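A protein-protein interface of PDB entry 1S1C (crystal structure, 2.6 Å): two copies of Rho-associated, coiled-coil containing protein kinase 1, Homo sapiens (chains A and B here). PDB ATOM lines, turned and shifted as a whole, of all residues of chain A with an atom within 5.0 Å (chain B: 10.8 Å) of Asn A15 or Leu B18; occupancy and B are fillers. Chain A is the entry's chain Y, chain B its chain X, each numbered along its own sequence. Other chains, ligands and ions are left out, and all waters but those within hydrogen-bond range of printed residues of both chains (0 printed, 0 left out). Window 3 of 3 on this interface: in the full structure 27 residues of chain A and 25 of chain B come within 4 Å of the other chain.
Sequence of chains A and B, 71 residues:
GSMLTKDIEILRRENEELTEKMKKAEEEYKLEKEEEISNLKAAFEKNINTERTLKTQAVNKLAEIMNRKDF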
ATOM      1  N   LEU A  11     -23.142  21.794 -14.231  1.00  0.00           N
ATOM      2  CA  LEU A  11     -23.288  22.621 -13.043  1.00  0.00           C
ATOM      3  C   LEU A  11     -22.996  24.078 -13.361  1.00  0.00           C
ATOM      4  O   LEU A  11     -23.361  24.969 -12.599  1.00  0.00           O
ATOM      5  CB  LEU A  11     -22.369  22.144 -11.923  1.00  0.00           C
ATOM      6  CG  LEU A  11     -22.932  21.003 -11.078  1.00  0.00           C
ATOM      7  CD1 LEU A  11     -23.141  19.761 -11.944  1.00  0.00           C
ATOM      8  CD2 LEU A  11     -21.978  20.710  -9.936  1.00  0.00           C
ATOM      9  N   ARG A  12     -22.332  24.318 -14.489  1.00  0.00           N
ATOM     10  CA  ARG A  12     -22.020  25.680 -14.899  1.00  0.00           C
ATOM     11  C   ARG A  12     -23.250  26.349 -15.503  1.00  0.00           C
ATOM     12  O   ARG A  12     -23.626  27.441 -15.085  1.00  0.00           O
ATOM     13  CB  ARG A  12     -20.853  25.705 -15.899  1.00  0.00           C
ATOM     14  CG  ARG A  12     -19.475  25.711 -15.237  1.00  0.00           C
ATOM     15  CD  ARG A  12     -18.554  26.759 -15.857  1.00  0.00           C
ATOM     16  NE  ARG A  12     -17.788  26.239 -16.984  1.00  0.00           N
ATOM     17  CZ  ARG A  12     -16.575  25.699 -16.882  1.00  0.00           C
ATOM     18  NH1 ARG A  12     -15.979  25.610 -15.698  1.00  0.00           N
ATOM     19  NH2 ARG A  12     -15.956  25.248 -17.965  1.00  0.00           N
ATOM     20  N   ARG A  13     -23.883  25.698 -16.475  1.00  0.00           N
ATOM     21  CA  ARG A  13     -25.077  26.263 -17.096  1.00  0.00           C
ATOM     22  C   ARG A  13     -26.143  26.437 -16.023  1.00  0.00           C
ATOM     23  O   ARG A  13     -26.957  27.361 -16.079  1.00  0.00           O
ATOM     24  CB  ARG A  13     -25.599  25.341 -18.198  1.00  0.00           C
ATOM     25  CG  ARG A  13     -24.586  25.071 -19.297  1.00  0.00           C
ATOM     26  CD  ARG A  13     -25.232  24.322 -20.447  1.00  0.00           C
ATOM     27  NE  ARG A  13     -24.243  23.792 -21.383  1.00  0.00           N
ATOM     28  CZ  ARG A  13     -24.550  23.131 -22.495  1.00  0.00           C
ATOM     29  NH1 ARG A  13     -25.821  22.924 -22.818  1.00  0.00           N
ATOM     30  NH2 ARG A  13     -23.588  22.667 -23.283  1.00  0.00           N
ATOM     31  N   GLU A  14     -26.115  25.539 -15.044  1.00  0.00           N
ATOM     32  CA  GLU A  14     -27.045  25.556 -13.923  1.00  0.00           C
ATOM     33  C   GLU A  14     -26.819  26.792 -13.050  1.00  0.00           C
ATOM     34  O   GLU A  14     -27.764  27.367 -12.508  1.00  0.00           O
ATOM     35  CB  GLU A  14     -26.862  24.276 -13.111  1.00  0.00           C
ATOM     36  CG  GLU A  14     -27.402  24.303 -11.700  1.00  0.00           C
ATOM     37  CD  GLU A  14     -27.256  22.952 -11.022  1.00  0.00           C
ATOM     38  OE1 GLU A  14     -27.368  22.887  -9.778  1.00  0.00           O
ATOM     39  OE2 GLU A  14     -27.035  21.950 -11.742  1.00  0.00           O
ATOM     40  N   ASN A  15     -25.558  27.191 -12.912  1.00  0.00           N
ATOM     41  CA  ASN A  15     -25.209  28.370 -12.131  1.00  0.00           C
ATOM     42  C   ASN A  15     -25.785  29.533 -12.926  1.00  0.00           C
ATOM     43  O   ASN A  15     -26.491  30.385 -12.389  1.00  0.00           O
ATOM     44  CB  ASN A  15     -23.680  28.496 -12.029  1.00  0.00           C
ATOM     45  CG  ASN A  15     -23.229  29.673 -11.162  1.00  0.00           C
ATOM     46  OD1 ASN A  15     -22.789  30.753 -11.810  1.00  0.00           O
ATOM     47  ND2 ASN A  15     -23.272  29.608  -9.930  1.00  0.00           N
ATOM     48  N   GLU A  16     -25.484  29.537 -14.220  1.00  0.00           N
ATOM     49  CA  GLU A  16     -25.943  30.566 -15.143  1.00  0.00           C
ATOM     50  C   GLU A  16     -27.453  30.734 -15.098  1.00  0.00           C
ATOM     51  O   GLU A  16     -27.960  31.803 -14.759  1.00  0.00           O
ATOM     52  CB  GLU A  16     -25.527  30.209 -16.571  1.00  0.00           C
ATOM     53  CG  GLU A  16     -24.028  30.244 -16.830  1.00  0.00           C
ATOM     54  CD  GLU A  16     -23.660  29.599 -18.158  1.00  0.00           C
ATOM     55  OE1 GLU A  16     -24.329  29.903 -19.174  1.00  0.00           O
ATOM     56  OE2 GLU A  16     -22.701  28.793 -18.182  1.00  0.00           O
ATOM     57  N   GLU A  17     -28.165  29.672 -15.453  1.00  0.00           N
ATOM     58  CA  GLU A  17     -29.622  29.691 -15.465  1.00  0.00           C
ATOM     59  C   GLU A  17     -30.188  30.220 -14.151  1.00  0.00           C
ATOM     60  O   GLU A  17     -31.088  31.057 -14.142  1.00  0.00           O
ATOM     61  CB  GLU A  17     -30.148  28.282 -15.752  1.00  0.00           C
ATOM     62  CG  GLU A  17     -29.777  27.780 -17.149  1.00  0.00           C
ATOM     63  CD  GLU A  17     -29.967  26.280 -17.327  1.00  0.00           C
ATOM     64  OE1 GLU A  17     -29.741  25.789 -18.455  1.00  0.00           O
ATOM     65  OE2 GLU A  17     -30.333  25.591 -16.347  1.00  0.00           O
ATOM     66  N   LEU A  18     -29.642  29.732 -13.044  1.00  0.00           N
ATOM     67  CA  LEU A  18     -30.073  30.149 -11.719  1.00  0.00           C
ATOM     68  C   LEU A  18     -29.870  31.655 -11.569  1.00  0.00           C
ATOM     69  O   LEU A  18     -30.636  32.335 -10.882  1.00  0.00           O
ATOM     70  CB  LEU A  18     -29.261  29.387 -10.674  1.00  0.00           C
ATOM     71  CG  LEU A  18     -29.506  29.608  -9.184  1.00  0.00           C
ATOM     72  CD1 LEU A  18     -28.742  28.558  -8.387  1.00  0.00           C
ATOM     73  CD2 LEU A  18     -29.053  30.991  -8.788  1.00  0.00           C
ATOM     74  N   THR A  19     -28.836  32.174 -12.223  1.00  0.00           N
ATOM     75  CA  THR A  19     -28.528  33.598 -12.164  1.00  0.00           C
ATOM     76  C   THR A  19     -29.524  34.387 -12.989  1.00  0.00           C
ATOM     77  O   THR A  19     -29.994  35.438 -12.568  1.00  0.00           O
ATOM     78  CB  THR A  19     -27.109  33.892 -12.693  1.00  0.00           C
ATOM     79  OG1 THR A  19     -26.141  33.287 -11.829  1.00  0.00           O
ATOM     80  CG2 THR A  19     -26.859  35.396 -12.750  1.00  0.00           C
ATOM     81  N   ASP B   7     -13.173  20.521  -7.682  1.00  0.00           N
ATOM     82  CA  ASP B   7     -13.794  21.542  -8.523  1.00  0.00           C
ATOM     83  C   ASP B   7     -15.304  21.360  -8.560  1.00  0.00           C
ATOM     84  O   ASP B   7     -16.054  22.330  -8.580  1.00  0.00           O
ATOM     85  CB  ASP B   7     -13.221  21.514  -9.947  1.00  0.00           C
ATOM     86  CG  ASP B   7     -11.804  22.084 -10.028  1.00  0.00           C
ATOM     87  OD1 ASP B   7     -11.488  23.037  -9.272  1.00  0.00           O
ATOM     88  OD2 ASP B   7     -11.008  21.592 -10.862  1.00  0.00           O
ATOM     89  N   ILE B   8     -15.743  20.109  -8.564  1.00  0.00           N
ATOM     90  CA  ILE B   8     -17.165  19.820  -8.568  1.00  0.00           C
ATOM     91  C   ILE B   8     -17.790  20.292  -7.258  1.00  0.00           C
ATOM     92  O   ILE B   8     -18.800  21.003  -7.262  1.00  0.00           O
ATOM     93  CB  ILE B   8     -17.424  18.309  -8.735  1.00  0.00           C
ATOM     94  CG1 ILE B   8     -17.037  17.877 -10.148  1.00  0.00           C
ATOM     95  CG2 ILE B   8     -18.885  17.994  -8.464  1.00  0.00           C
ATOM     96  CD1 ILE B   8     -17.012  16.388 -10.333  1.00  0.00           C
ATOM     97  N   GLU B   9     -17.191  19.892  -6.141  1.00  0.00           N
ATOM     98  CA  GLU B   9     -17.696  20.277  -4.826  1.00  0.00           C
ATOM     99  C   GLU B   9     -17.802  21.799  -4.699  1.00  0.00           C
ATOM    100  O   GLU B   9     -18.826  22.312  -4.261  1.00  0.00           O
ATOM    101  CB  GLU B   9     -16.800  19.716  -3.735  1.00  0.00           C
ATOM    102  N   ILE B  10     -16.748  22.513  -5.094  1.00  0.00           N
ATOM    103  CA  ILE B  10     -16.731  23.975  -5.026  1.00  0.00           C
ATOM    104  C   ILE B  10     -17.845  24.600  -5.877  1.00  0.00           C
ATOM    105  O   ILE B  10     -18.347  25.682  -5.558  1.00  0.00           O
ATOM    106  CB  ILE B  10     -15.355  24.533  -5.491  1.00  0.00           C
ATOM    107  CG1 ILE B  10     -14.312  24.326  -4.393  1.00  0.00           C
ATOM    108  CG2 ILE B  10     -15.464  26.007  -5.844  1.00  0.00           C
ATOM    109  CD1 ILE B  10     -12.900  24.692  -4.818  1.00  0.00           C
ATOM    110  N   LEU B  11     -18.224  23.917  -6.955  1.00  0.00           N
ATOM    111  CA  LEU B  11     -19.276  24.399  -7.841  1.00  0.00           C
ATOM    112  C   LEU B  11     -20.658  24.179  -7.242  1.00  0.00           C
ATOM    113  O   LEU B  11     -21.542  25.024  -7.392  1.00  0.00           O
ATOM    114  CB  LEU B  11     -19.190  23.705  -9.197  1.00  0.00           C
ATOM    115  CG  LEU B  11     -18.798  24.632 -10.349  1.00  0.00           C
ATOM    116  CD1 LEU B  11     -18.458  23.808 -11.575  1.00  0.00           C
ATOM    117  CD2 LEU B  11     -19.937  25.594 -10.641  1.00  0.00           C
ATOM    118  N   ARG B  12     -20.850  23.046  -6.574  1.00  0.00           N
ATOM    119  CA  ARG B  12     -22.137  22.758  -5.945  1.00  0.00           C
ATOM    120  C   ARG B  12     -22.338  23.702  -4.769  1.00  0.00           C
ATOM    121  O   ARG B  12     -23.458  23.923  -4.327  1.00  0.00           O
ATOM    122  CB  ARG B  12     -22.213  21.311  -5.437  1.00  0.00           C
ATOM    123  CG  ARG B  12     -22.210  20.254  -6.525  1.00  0.00           C
ATOM    124  CD  ARG B  12     -23.142  19.090  -6.177  1.00  0.00           C
ATOM    125  NE  ARG B  12     -23.194  18.093  -7.246  1.00  0.00           N
ATOM    126  CZ  ARG B  12     -22.311  17.106  -7.407  1.00  0.00           C
ATOM    127  NH1 ARG B  12     -21.298  16.970  -6.554  1.00  0.00           N
ATOM    128  NH2 ARG B  12     -22.427  16.269  -8.440  1.00  0.00           N
ATOM    129  N   ARG B  13     -21.244  24.259  -4.264  1.00  0.00           N
ATOM    130  CA  ARG B  13     -21.322  25.179  -3.141  1.00  0.00           C
ATOM    131  C   ARG B  13     -21.647  26.603  -3.597  1.00  0.00           C
ATOM    132  O   ARG B  13     -22.459  27.282  -2.972  1.00  0.00           O
ATOM    133  CB  ARG B  13     -20.013  25.150  -2.354  1.00  0.00           C
ATOM    134  CG  ARG B  13     -19.962  26.128  -1.201  1.00  0.00           C
ATOM    135  CD  ARG B  13     -18.670  25.975  -0.427  1.00  0.00           C
ATOM    136  NE  ARG B  13     -18.446  27.090   0.491  1.00  0.00           N
ATOM    137  CZ  ARG B  13     -17.447  27.145   1.369  1.00  0.00           C
ATOM    138  NH1 ARG B  13     -16.581  26.140   1.449  1.00  0.00           N
ATOM    139  NH2 ARG B  13     -17.309  28.204   2.162  1.00  0.00           N
ATOM    140  N   GLU B  14     -21.020  27.052  -4.683  1.00  0.00           N
ATOM    141  CA  GLU B  14     -21.279  28.392  -5.218  1.00  0.00           C
ATOM    142  C   GLU B  14     -22.720  28.496  -5.688  1.00  0.00           C
ATOM    143  O   GLU B  14     -23.410  29.460  -5.380  1.00  0.00           O
ATOM    144  CB  GLU B  14     -20.345  28.693  -6.388  1.00  0.00           C
ATOM    145  CG  GLU B  14     -18.976  29.189  -5.966  1.00  0.00           C
ATOM    146  CD  GLU B  14     -17.952  29.088  -7.079  1.00  0.00           C
ATOM    147  OE1 GLU B  14     -18.264  29.500  -8.218  1.00  0.00           O
ATOM    148  OE2 GLU B  14     -16.834  28.598  -6.809  1.00  0.00           O
ATOM    149  N   ASN B  15     -23.161  27.499  -6.444  1.00  0.00           N
ATOM    150  CA  ASN B  15     -24.525  27.460  -6.950  1.00  0.00           C
ATOM    151  C   ASN B  15     -25.492  27.412  -5.767  1.00  0.00           C
ATOM    152  O   ASN B  15     -26.621  27.890  -5.840  1.00  0.00           O
ATOM    153  CB  ASN B  15     -24.719  26.221  -7.832  1.00  0.00           C
ATOM    154  CG  ASN B  15     -24.147  26.399  -9.235  1.00  0.00           C
ATOM    155  OD1 ASN B  15     -22.970  26.722  -9.418  1.00  0.00           O
ATOM    156  ND2 ASN B  15     -24.985  26.178 -10.232  1.00  0.00           N
ATOM    157  N   GLU B  16     -25.019  26.836  -4.674  1.00  0.00           N
ATOM    158  CA  GLU B  16     -25.795  26.689  -3.450  1.00  0.00           C
ATOM    159  C   GLU B  16     -25.829  28.013  -2.675  1.00  0.00           C
ATOM    160  O   GLU B  16     -26.878  28.454  -2.203  1.00  0.00           O
ATOM    161  CB  GLU B  16     -25.146  25.590  -2.608  1.00  0.00           C
ATOM    162  CG  GLU B  16     -25.858  25.201  -1.333  1.00  0.00           C
ATOM    163  CD  GLU B  16     -25.125  24.080  -0.606  1.00  0.00           C
ATOM    164  OE1 GLU B  16     -24.893  23.019  -1.232  1.00  0.00           O
ATOM    165  OE2 GLU B  16     -24.776  24.257   0.585  1.00  0.00           O
ATOM    166  N   GLU B  17     -24.667  28.641  -2.549  1.00  0.00           N
ATOM    167  CA  GLU B  17     -24.566  29.902  -1.842  1.00  0.00           C
ATOM    168  C   GLU B  17     -25.291  30.959  -2.653  1.00  0.00           C
ATOM    169  O   GLU B  17     -25.792  31.946  -2.110  1.00  0.00           O
ATOM    170  CB  GLU B  17     -23.098  30.274  -1.660  1.00  0.00           C
ATOM    171  CG  GLU B  17     -22.321  29.204  -0.907  1.00  0.00           C
ATOM    172  CD  GLU B  17     -20.840  29.505  -0.809  1.00  0.00           C
ATOM    173  OE1 GLU B  17     -20.232  29.809  -1.860  1.00  0.00           O
ATOM    174  OE2 GLU B  17     -20.289  29.432   0.314  1.00  0.00           O
ATOM    175  N   LEU B  18     -25.354  30.732  -3.960  1.00  0.00           N
ATOM    176  CA  LEU B  18     -26.018  31.645  -4.877  1.00  0.00           C
ATOM    177  C   LEU B  18     -27.523  31.631  -4.604  1.00  0.00           C
ATOM    178  O   LEU B  18     -28.188  32.665  -4.677  1.00  0.00           O
ATOM    179  CB  LEU B  18     -25.748  31.212  -6.318  1.00  0.00           C
ATOM    180  CG  LEU B  18     -25.772  32.281  -7.411  1.00  0.00           C
ATOM    181  CD1 LEU B  18     -25.680  31.588  -8.761  1.00  0.00           C
ATOM    182  CD2 LEU B  18     -27.040  33.122  -7.331  1.00  0.00           C
ATOM    183  N   THR B  19     -28.044  30.446  -4.291  1.00  0.00           N
ATOM    184  CA  THR B  19     -29.465  30.252  -3.996  1.00  0.00           C
ATOM    185  C   THR B  19     -29.831  30.923  -2.675  1.00  0.00           C
ATOM    186  O   THR B  19     -31.002  31.202  -2.405  1.00  0.00           O
ATOM    187  CB  THR B  19     -29.814  28.739  -3.897  1.00  0.00           C
ATOM    188  OG1 THR B  19     -29.615  28.116  -5.170  1.00  0.00           O
ATOM    189  CG2 THR B  19     -31.259  28.541  -3.468  1.00  0.00           C
ATOM    190  N   GLU B  20     -28.821  31.170  -1.853  1.00  0.00           N
ATOM    191  CA  GLU B  20     -29.035  31.802  -0.564  1.00  0.00           C
ATOM    192  C   GLU B  20     -28.882  33.300  -0.750  1.00  0.00           C
ATOM    193  O   GLU B  20     -29.272  34.089   0.104  1.00  0.00           O
ATOM    194  CB  GLU B  20     -28.020  31.273   0.445  1.00  0.00           C
ATOM    195  CG  GLU B  20     -28.545  31.215   1.862  1.00  0.00           C
ATOM    196  CD  GLU B  20     -27.628  30.440   2.791  1.00  0.00           C
ATOM    197  OE1 GLU B  20     -27.963  30.328   3.994  1.00  0.00           O
ATOM    198  OE2 GLU B  20     -26.580  29.940   2.318  1.00  0.00           O
ATOM    199  N   LYS B  21     -28.310  33.680  -1.888  1.00  0.00           N
ATOM    200  CA  LYS B  21     -28.119  35.083  -2.221  1.00  0.00           C
ATOM    201  C   LYS B  21     -29.299  35.488  -3.093  1.00  0.00           C
ATOM    202  O   LYS B  21     -29.256  36.489  -3.803  1.00  0.00           O
ATOM    203  CB  LYS B  21     -26.810  35.281  -2.985  1.00  0.00           C
ATOM    204  CG  LYS B  21     -26.393  36.733  -3.111  1.00  0.00           C
ATOM    205  CD  LYS B  21     -25.097  36.884  -3.900  1.00  0.00           C
ATOM    206  CE  LYS B  21     -24.688  38.350  -4.015  1.00  0.00           C
ATOM    207  NZ  LYS B  21     -23.455  38.535  -4.834  1.00  0.00           N
ATOM    208  N   MET B  22     -30.345  34.671  -3.044  1.00  0.00           N
ATOM    209  CA  MET B  22     -31.567  34.923  -3.793  1.00  0.00           C
ATOM    210  C   MET B  22     -32.700  35.012  -2.788  1.00  0.00           C
ATOM    211  O   MET B  22     -33.390  36.023  -2.711  1.00  0.00           O
ATOM    212  CB  MET B  22     -31.870  33.786  -4.762  1.00  0.00           C
ATOM    213  CG  MET B  22     -30.843  33.571  -5.853  1.00  0.00           C
ATOM    214  SD  MET B  22     -31.463  32.447  -7.143  1.00  0.00           S
ATOM    215  CE  MET B  22     -32.987  31.786  -6.374  1.00  0.00           C
ATOM    216  N   LYS B  23     -32.886  33.940  -2.024  1.00  0.00           N
ATOM    217  CA  LYS B  23     -33.935  33.901  -1.014  1.00  0.00           C
ATOM    218  C   LYS B  23     -33.786  35.028   0.001  1.00  0.00           C
ATOM    219  O   LYS B  23     -34.777  35.566   0.490  1.00  0.00           O
ATOM    220  CB  LYS B  23     -33.932  32.563  -0.278  1.00  0.00           C
ATOM    221  CG  LYS B  23     -34.627  31.437  -1.011  1.00  0.00           C
ATOM    222  CD  LYS B  23     -34.817  30.251  -0.078  1.00  0.00           C
ATOM    223  CE  LYS B  23     -35.607  29.127  -0.730  1.00  0.00           C
ATOM    224  NZ  LYS B  23     -35.869  28.018   0.234  1.00  0.00           N
ATOM    225  N   LYS B  24     -32.545  35.378   0.319  1.00  0.00           N
ATOM    226  CA  LYS B  24     -32.282  36.445   1.275  1.00  0.00           C
ATOM    227  C   LYS B  24     -31.983  37.738   0.525  1.00  0.00           C
ATOM    228  O   LYS B  24     -31.524  38.723   1.100  1.00  0.00           O
ATOM    229  CB  LYS B  24     -31.117  36.052   2.191  1.00  0.00           C
ATOM    230  CG  LYS B  24     -31.372  34.750   2.960  1.00  0.00           C
ATOM    231  CD  LYS B  24     -30.184  34.335   3.812  1.00  0.00           C
ATOM    232  CE  LYS B  24     -28.935  34.171   2.962  1.00  0.00           C
ATOM    233  NZ  LYS B  24     -27.773  33.685   3.746  1.00  0.00           N
ATOM    234  N   ALA B  25     -32.247  37.713  -0.777  1.00  0.00           N
ATOM    235  CA  ALA B  25     -32.054  38.869  -1.641  1.00  0.00           C
ATOM    236  C   ALA B  25     -33.447  39.442  -1.837  1.00  0.00           C
ATOM    237  O   ALA B  25     -33.650  40.654  -1.804  1.00  0.00           O
ATOM    238  CB  ALA B  25     -31.473  38.433  -2.975  1.00  0.00           C
ATOM    239  N   GLU B  26     -34.401  38.538  -2.043  1.00  0.00           N
ATOM    240  CA  GLU B  26     -35.804  38.885  -2.225  1.00  0.00           C
ATOM    241  C   GLU B  26     -36.333  39.361  -0.876  1.00  0.00           C
ATOM    242  O   GLU B  26     -37.006  40.385  -0.794  1.00  0.00           O
ATOM    243  CB  GLU B  26     -36.589  37.656  -2.702  1.00  0.00           C
ATOM    244  CG  GLU B  26     -36.257  36.388  -1.918  1.00  0.00           C
ATOM    245  CD  GLU B  26     -37.062  35.169  -2.345  1.00  0.00           C
ATOM    246  OE1 GLU B  26     -37.109  34.877  -3.563  1.00  0.00           O
ATOM    247  OE2 GLU B  26     -37.633  34.497  -1.454  1.00  0.00           O
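Among the printed residues, merely in contact across the chains: Leu A18 with Met B22, Leu A18 with Leu B18, Asn A15 with Leu B18, Leu A18 with Thr B19, Leu A18 with Asn B15, Glu A14 with Asn B15, Leu A11 with Arg B12, Thr A19 with Leu B18 and Leu A11 with Leu B11.
Leu A11 touches Arg B12, but with the chains exchanged Arg A12 does not touch Leu B11 (4.3 Å). Glu A14 touches Asn B15, but with the chains exchanged Asn A15 does not touch Glu B14 (4.4 Å). Asn A15 touches Leu B18, and with the chains exchanged Leu A18 touches Asn B15. Leu B18 touches its own counterpart, Leu A18. Positions printed for both chains: 11, 12, 13, 14, 15, 16, 17, 18 and 19. Of the 11 pairs that touch across the chains among the printed residues, 7 have their exchanged pair printed and touching as well.
Printed residues of chain A within 4 Å of Leu B18: Asn A15, Leu A18 and Thr A19. Glu A14 touches just one residue of chain B: Asn B15. Of chain B, only Asn B15, Leu B18, Thr B19 and Met B22 come within 4 Å of Leu A18. Of the printed residues of chain A, Met B22 touches Leu A18. Printed residues of chain A within 4 Å of Arg B12: Leu A11 (3.4 Å). Asp B7 touches none of the printed residues of chain A. The nearest residue of chain B that does not touch Asn A15 is Glu B14 (4.4 Å). The nearest printed residue of chain A that does not touch Leu B18 is Glu A16 (5.8 Å). The nearest printed residue of chain A that does not touch Arg B12 is Glu A14 (6.5 Å).
Hydrophobic or aromatic side chains of chain B within 4 Å of the printed part of chain A: Leu B11, Leu B18 and Met B22. Of the 9 printed residues of chain A, 5 touch a printed residue of chain B. Printed residues of chain A that touch a printed residue of chain B: Leu A11, Glu A14, Asn A15, Leu A18 and Thr A19. Hydrophobic or aromatic side chains of chain A that line the printed part of chain B: Leu A11 and Leu A18. Among the printed residues, no Asp or Glu carboxylate lies within 4 Å of a Lys or Arg side-chain nitrogen of the other chain.
The backbone carbonyl oxygen (O) of Leu B11 sits close to the side-chain amide oxygen (OD1) of Asn B15 (3.0 Å). The backbone carbonyl oxygen of Asn B15 is in hydrogen-bond range of the side-chain hydroxyl of Thr B19, 3.1 Å away. OG1 of Thr A19 is in hydrogen-bond range of O of Asn A15 (3.0 Å).
O of Leu A11 lies within hydrogen-bond range of ND2 of Asn B15, 3.1 Å away. The side-chain amide nitrogen of Asn B15 lies close to the backbone NH of Asn A15 (2.9 Å).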
